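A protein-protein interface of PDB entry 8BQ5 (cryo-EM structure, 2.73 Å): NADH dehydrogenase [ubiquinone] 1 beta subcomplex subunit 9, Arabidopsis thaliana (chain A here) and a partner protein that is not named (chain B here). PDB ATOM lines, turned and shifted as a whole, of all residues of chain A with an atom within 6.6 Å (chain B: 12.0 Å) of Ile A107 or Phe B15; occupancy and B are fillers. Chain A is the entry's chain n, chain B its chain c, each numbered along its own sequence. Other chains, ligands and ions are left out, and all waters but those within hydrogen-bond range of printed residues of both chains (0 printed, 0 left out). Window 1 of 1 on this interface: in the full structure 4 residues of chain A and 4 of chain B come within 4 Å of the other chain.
Among the printed residues, pairs that only touch across the chains: Pro A101 with Arg B16 (3.3 Å), Pro A101 with Phe B15 (3.4 Å), Ile A107 with Lys B18 (3.6 Å), Ile A105 with Phe B15 (3.6 Å), Pro A101 with Gly B13 (3.8 Å) and Ile A107 with Phe B15 (3.99 Å).
The side-chain hydroxyl (OH) of Tyr A109 sits close to the backbone carbonyl oxygen (O) of Lys B18 (3.2 Å).
Of the printed residues of chain B, Ile A107 touches Phe B15 and Lys B18.
Printed residues of chain A within 4 Å of Phe B15: Pro A101, Ile A105 and Ile A107.
No residue of chain B comes within 4 Å of Pro A102.
No residue of chain B comes within 4 Å of Ala A103.
Ile A105 touches just one residue of chain B: Phe B15 (3.6 Å).
No residue of chain B comes within 4 Å of Val A108.
Of chain B, only Lys B18 comes within 4 Å of Tyr A109.
Of the printed residues of chain A, Arg B16 touches Pro A101.
Of the printed residues of chain A, Gly B13 touches Pro A101 (3.8 Å).
Of the printed residues of chain A, Lys B18 touches Ile A107 (3.6 Å) and Tyr A109 (3.2 Å).
Trp B20 touches none of the printed residues of chain A.
The nearest printed residue of chain A that does not touch Phe B15 is Pro A102 (4.1 Å).
The nearest printed residue of chain A that does not touch Gly B13 is Pro A102 (7.8 Å).
Of the 13 printed residues of chain B, 4 touch a printed residue of chain A.
Printed residues of chain B that touch a printed residue of chain A: Gly B13, Phe B15, Arg B16 and Lys B18.
Hydrophobic or aromatic side chains of chain B that line the printed part of chain A: Phe B15.
Among the printed residues, no Asp or Glu carboxylate lies within 4 Å of a Lys or Arg side-chain nitrogen of the other chain.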
ATOM      1  N   PRO A 101     -12.719 -26.629  -9.049  1.00  0.00           N
ATOM      2  CA  PRO A 101     -12.186 -25.373  -9.574  1.00  0.00           C
ATOM      3  C   PRO A 101     -10.727 -25.523  -9.962  1.00  0.00           C
ATOM      4  O   PRO A 101      -9.961 -26.235  -9.291  1.00  0.00           O
ATOM      5  CB  PRO A 101     -12.353 -24.395  -8.396  1.00  0.00           C
ATOM      6  CG  PRO A 101     -13.263 -25.063  -7.435  1.00  0.00           C
ATOM      7  CD  PRO A 101     -13.121 -26.529  -7.639  1.00  0.00           C
ATOM      8  N   PRO A 102     -10.293 -24.868 -11.037  1.00  0.00           N
ATOM      9  CA  PRO A 102      -8.885 -24.958 -11.429  1.00  0.00           C
ATOM     10  C   PRO A 102      -7.980 -24.258 -10.428  1.00  0.00           C
ATOM     11  O   PRO A 102      -8.376 -23.307  -9.749  1.00  0.00           O
ATOM     12  CB  PRO A 102      -8.860 -24.254 -12.789  1.00  0.00           C
ATOM     13  CG  PRO A 102      -9.929 -23.220 -12.645  1.00  0.00           C
ATOM     14  CD  PRO A 102     -11.037 -23.960 -11.927  1.00  0.00           C
ATOM     15  N   ALA A 103      -6.753 -24.751 -10.336  1.00  0.00           N
ATOM     16  CA  ALA A 103      -5.741 -24.118  -9.508  1.00  0.00           C
ATOM     17  C   ALA A 103      -5.076 -22.976 -10.269  1.00  0.00           C
ATOM     18  O   ALA A 103      -5.142 -22.892 -11.498  1.00  0.00           O
ATOM     19  CB  ALA A 103      -4.693 -25.135  -9.058  1.00  0.00           C
ATOM     20  N   ILE A 105      -5.772 -19.632  -9.578  1.00  0.00           N
ATOM     21  CA  ILE A 105      -6.693 -18.509  -9.696  1.00  0.00           C
ATOM     22  C   ILE A 105      -6.446 -17.570  -8.525  1.00  0.00           C
ATOM     23  O   ILE A 105      -6.374 -18.007  -7.371  1.00  0.00           O
ATOM     24  CB  ILE A 105      -8.156 -18.976  -9.730  1.00  0.00           C
ATOM     25  CG1 ILE A 105      -8.398 -19.905 -10.921  1.00  0.00           C
ATOM     26  CG2 ILE A 105      -9.094 -17.778  -9.793  1.00  0.00           C
ATOM     27  CD1 ILE A 105      -7.873 -19.380 -12.231  1.00  0.00           C
ATOM     28  N   GLU A 106      -6.313 -16.284  -8.819  1.00  0.00           N
ATOM     29  CA  GLU A 106      -6.085 -15.264  -7.810  1.00  0.00           C
ATOM     30  C   GLU A 106      -7.219 -14.251  -7.833  1.00  0.00           C
ATOM     31  O   GLU A 106      -7.715 -13.880  -8.901  1.00  0.00           O
ATOM     32  CB  GLU A 106      -4.737 -14.576  -8.031  1.00  0.00           C
ATOM     33  CG  GLU A 106      -3.769 -15.432  -8.822  1.00  0.00           C
ATOM     34  CD  GLU A 106      -2.375 -14.857  -8.893  1.00  0.00           C
ATOM     35  OE1 GLU A 106      -2.106 -14.031  -9.775  1.00  0.00           O
ATOM     36  OE2 GLU A 106      -1.526 -15.237  -8.069  1.00  0.00           O
ATOM     37  N   ILE A 107      -7.641 -13.826  -6.647  1.00  0.00           N
ATOM     38  CA  ILE A 107      -8.682 -12.821  -6.482  1.00  0.00           C
ATOM     39  C   ILE A 107      -8.031 -11.570  -5.909  1.00  0.00           C
ATOM     40  O   ILE A 107      -7.416 -11.620  -4.837  1.00  0.00           O
ATOM     41  CB  ILE A 107      -9.811 -13.326  -5.566  1.00  0.00           C
ATOM     42  CG1 ILE A 107     -10.402 -14.634  -6.099  1.00  0.00           C
ATOM     43  CG2 ILE A 107     -10.891 -12.270  -5.423  1.00  0.00           C
ATOM     44  CD1 ILE A 107     -10.848 -14.577  -7.541  1.00  0.00           C
ATOM     45  N   VAL A 108      -8.164 -10.454  -6.622  1.00  0.00           N
ATOM     46  CA  VAL A 108      -7.548  -9.188  -6.234  1.00  0.00           C
ATOM     47  C   VAL A 108      -8.539  -8.380  -5.415  1.00  0.00           C
ATOM     48  O   VAL A 108      -9.717  -8.260  -5.778  1.00  0.00           O
ATOM     49  CB  VAL A 108      -7.084  -8.386  -7.463  1.00  0.00           C
ATOM     50  CG1 VAL A 108      -6.303  -7.157  -7.027  1.00  0.00           C
ATOM     51  CG2 VAL A 108      -6.243  -9.250  -8.371  1.00  0.00           C
ATOM     52  N   TYR A 109      -8.066  -7.823  -4.308  1.00  0.00           N
ATOM     53  CA  TYR A 109      -8.842  -6.892  -3.508  1.00  0.00           C
ATOM     54  C   TYR A 109      -8.349  -5.476  -3.771  1.00  0.00           C
ATOM     55  O   TYR A 109      -7.261  -5.275  -4.316  1.00  0.00           O
ATOM     56  CB  TYR A 109      -8.723  -7.214  -2.018  1.00  0.00           C
ATOM     57  CG  TYR A 109      -9.311  -8.543  -1.621  1.00  0.00           C
ATOM     58  CD1 TYR A 109     -10.429  -9.055  -2.266  1.00  0.00           C
ATOM     59  CD2 TYR A 109      -8.744  -9.290  -0.601  1.00  0.00           C
ATOM     60  CE1 TYR A 109     -10.964 -10.273  -1.900  1.00  0.00           C
ATOM     61  CE2 TYR A 109      -9.270 -10.503  -0.229  1.00  0.00           C
ATOM     62  CZ  TYR A 109     -10.378 -10.992  -0.880  1.00  0.00           C
ATOM     63  OH  TYR A 109     -10.901 -12.206  -0.504  1.00  0.00           O
ATOM     64  N   GLY B  13     -14.429 -24.118  -3.500  1.00  0.00           N
ATOM     65  CA  GLY B  13     -13.161 -24.800  -3.679  1.00  0.00           C
ATOM     66  C   GLY B  13     -12.029 -24.145  -2.911  1.00  0.00           C
ATOM     67  O   GLY B  13     -11.948 -24.263  -1.689  1.00  0.00           O
ATOM     68  N   ASP B  14     -11.146 -23.458  -3.633  1.00  0.00           N
ATOM     69  CA  ASP B  14     -10.052 -22.713  -3.027  1.00  0.00           C
ATOM     70  C   ASP B  14     -10.178 -21.212  -3.232  1.00  0.00           C
ATOM     71  O   ASP B  14     -10.211 -20.457  -2.256  1.00  0.00           O
ATOM     72  CB  ASP B  14      -8.709 -23.204  -3.587  1.00  0.00           C
ATOM     73  CG  ASP B  14      -8.345 -24.587  -3.095  1.00  0.00           C
ATOM     74  OD1 ASP B  14      -8.964 -25.054  -2.116  1.00  0.00           O
ATOM     75  OD2 ASP B  14      -7.443 -25.212  -3.688  1.00  0.00           O
ATOM     76  N   PHE B  15     -10.257 -20.752  -4.483  1.00  0.00           N
ATOM     77  CA  PHE B  15     -10.409 -19.323  -4.724  1.00  0.00           C
ATOM     78  C   PHE B  15     -11.826 -18.846  -4.434  1.00  0.00           C
ATOM     79  O   PHE B  15     -12.021 -17.675  -4.092  1.00  0.00           O
ATOM     80  CB  PHE B  15      -9.999 -18.974  -6.160  1.00  0.00           C
ATOM     81  CG  PHE B  15     -10.973 -19.432  -7.212  1.00  0.00           C
ATOM     82  CD1 PHE B  15     -12.054 -18.642  -7.576  1.00  0.00           C
ATOM     83  CD2 PHE B  15     -10.795 -20.644  -7.852  1.00  0.00           C
ATOM     84  CE1 PHE B  15     -12.942 -19.063  -8.544  1.00  0.00           C
ATOM     85  CE2 PHE B  15     -11.679 -21.066  -8.823  1.00  0.00           C
ATOM     86  CZ  PHE B  15     -12.754 -20.275  -9.167  1.00  0.00           C
ATOM     87  N   ARG B  16     -12.818 -19.731  -4.554  1.00  0.00           N
ATOM     88  CA  ARG B  16     -14.196 -19.341  -4.283  1.00  0.00           C
ATOM     89  C   ARG B  16     -14.405 -18.930  -2.832  1.00  0.00           C
ATOM     90  O   ARG B  16     -15.395 -18.255  -2.529  1.00  0.00           O
ATOM     91  CB  ARG B  16     -15.145 -20.478  -4.661  1.00  0.00           C
ATOM     92  CG  ARG B  16     -14.900 -21.028  -6.057  1.00  0.00           C
ATOM     93  CD  ARG B  16     -16.034 -21.917  -6.525  1.00  0.00           C
ATOM     94  NE  ARG B  16     -15.961 -23.249  -5.938  1.00  0.00           N
ATOM     95  CZ  ARG B  16     -16.380 -24.354  -6.537  1.00  0.00           C
ATOM     96  NH1 ARG B  16     -16.899 -24.327  -7.753  1.00  0.00           N
ATOM     97  NH2 ARG B  16     -16.267 -25.518  -5.903  1.00  0.00           N
ATOM     98  N   ALA B  17     -13.496 -19.313  -1.934  1.00  0.00           N
ATOM     99  CA  ALA B  17     -13.540 -18.838  -0.558  1.00  0.00           C
ATOM    100  C   ALA B  17     -13.182 -17.364  -0.434  1.00  0.00           C
ATOM    101  O   ALA B  17     -13.491 -16.753   0.594  1.00  0.00           O
ATOM    102  CB  ALA B  17     -12.602 -19.672   0.315  1.00  0.00           C
ATOM    103  N   LYS B  18     -12.538 -16.781  -1.443  1.00  0.00           N
ATOM    104  CA  LYS B  18     -12.248 -15.356  -1.463  1.00  0.00           C
ATOM    105  C   LYS B  18     -13.198 -14.584  -2.367  1.00  0.00           C
ATOM    106  O   LYS B  18     -12.918 -13.431  -2.706  1.00  0.00           O
ATOM    107  CB  LYS B  18     -10.798 -15.113  -1.893  1.00  0.00           C
ATOM    108  CG  LYS B  18      -9.791 -16.048  -1.243  1.00  0.00           C
ATOM    109  CD  LYS B  18      -8.464 -15.348  -0.956  1.00  0.00           C
ATOM    110  CE  LYS B  18      -8.102 -14.318  -2.018  1.00  0.00           C
ATOM    111  NZ  LYS B  18      -7.346 -14.926  -3.147  1.00  0.00           N
ATOM    112  N   VAL B  19     -14.314 -15.191  -2.761  1.00  0.00           N
ATOM    113  CA  VAL B  19     -15.277 -14.573  -3.663  1.00  0.00           C
ATOM    114  C   VAL B  19     -16.556 -14.305  -2.883  1.00  0.00           C
ATOM    115  O   VAL B  19     -17.138 -15.224  -2.292  1.00  0.00           O
ATOM    116  CB  VAL B  19     -15.555 -15.455  -4.889  1.00  0.00           C
ATOM    117  CG1 VAL B  19     -16.768 -14.942  -5.645  1.00  0.00           C
ATOM    118  CG2 VAL B  19     -14.336 -15.504  -5.794  1.00  0.00           C
ATOM    119  N   TRP B  20     -16.992 -13.052  -2.888  1.00  0.00           N
ATOM    120  CA  TRP B  20     -18.221 -12.643  -2.224  1.00  0.00           C
ATOM    121  C   TRP B  20     -19.388 -12.734  -3.198  1.00  0.00           C
ATOM    122  O   TRP B  20     -19.301 -12.244  -4.326  1.00  0.00           O
ATOM    123  CB  TRP B  20     -18.084 -11.215  -1.695  1.00  0.00           C
ATOM    124  CG  TRP B  20     -19.185 -10.768  -0.784  1.00  0.00           C
ATOM    125  CD1 TRP B  20     -19.169 -10.770   0.578  1.00  0.00           C
ATOM    126  CD2 TRP B  20     -20.457 -10.228  -1.169  1.00  0.00           C
ATOM    127  NE1 TRP B  20     -20.353 -10.276   1.067  1.00  0.00           N
ATOM    128  CE2 TRP B  20     -21.160  -9.935   0.015  1.00  0.00           C
ATOM    129  CE3 TRP B  20     -21.070  -9.969  -2.399  1.00  0.00           C
ATOM    130  CZ2 TRP B  20     -22.444  -9.395   0.005  1.00  0.00           C
ATOM    131  CZ3 TRP B  20     -22.345  -9.435  -2.406  1.00  0.00           C
ATOM    132  CH2 TRP B  20     -23.019  -9.155  -1.212  1.00  0.00           C
ATOM    133  N   SER B  21     -20.475 -13.366  -2.759  1.00  0.00           N
ATOM    134  CA  SER B  21     -21.709 -13.409  -3.528  1.00  0.00           C
ATOM    135  C   SER B  21     -22.885 -13.216  -2.581  1.00  0.00           C
ATOM    136  O   SER B  21     -22.780 -13.447  -1.375  1.00  0.00           O
ATOM    137  CB  SER B  21     -21.865 -14.723  -4.305  1.00  0.00           C
ATOM    138  OG  SER B  21     -21.841 -15.838  -3.434  1.00  0.00           O
ATOM    139  N   GLY B  24     -24.340 -16.684  -1.406  1.00  0.00           N
ATOM    140  CA  GLY B  24     -23.519 -17.403  -0.458  1.00  0.00           C
ATOM    141  C   GLY B  24     -22.384 -18.199  -1.059  1.00  0.00           C
ATOM    142  O   GLY B  24     -21.390 -18.442  -0.364  1.00  0.00           O
ATOM    143  N   GLY B  25     -22.490 -18.604  -2.320  1.00  0.00           N
ATOM    144  CA  GLY B  25     -21.457 -19.387  -2.950  1.00  0.00           C
ATOM    145  C   GLY B  25     -21.626 -20.872  -2.703  1.00  0.00           C
ATOM    146  O   GLY B  25     -22.647 -21.328  -2.180  1.00  0.00           O
ATOM    147  N   PRO B  26     -20.621 -21.657  -3.079  1.00  0.00           N
ATOM    148  CA  PRO B  26     -20.719 -23.111  -2.915  1.00  0.00           C
ATOM    149  C   PRO B  26     -20.516 -23.528  -1.467  1.00  0.00           C
ATOM    150  O   PRO B  26     -19.570 -23.098  -0.802  1.00  0.00           O
ATOM    151  CB  PRO B  26     -19.596 -23.645  -3.810  1.00  0.00           C
ATOM    152  CG  PRO B  26     -18.597 -22.534  -3.873  1.00  0.00           C
ATOM    153  CD  PRO B  26     -19.310 -21.237  -3.606  1.00  0.00           C
ATOM    154  N   ASN B  27     -21.423 -24.382  -0.988  1.00  0.00           N
ATOM    155  CA  ASN B  27     -21.367 -24.937   0.366  1.00  0.00           C
ATOM    156  C   ASN B  27     -21.407 -23.834   1.422  1.00  0.00           C
ATOM    157  O   ASN B  27     -20.479 -23.663   2.213  1.00  0.00           O
ATOM    158  CB  ASN B  27     -20.128 -25.817   0.547  1.00  0.00           C
ATOM    159  CG  ASN B  27     -20.062 -26.945  -0.458  1.00  0.00           C
ATOM    160  OD1 ASN B  27     -20.998 -27.731  -0.590  1.00  0.00           O
ATOM    161  ND2 ASN B  27     -18.949 -27.028  -1.178  1.00  0.00           N
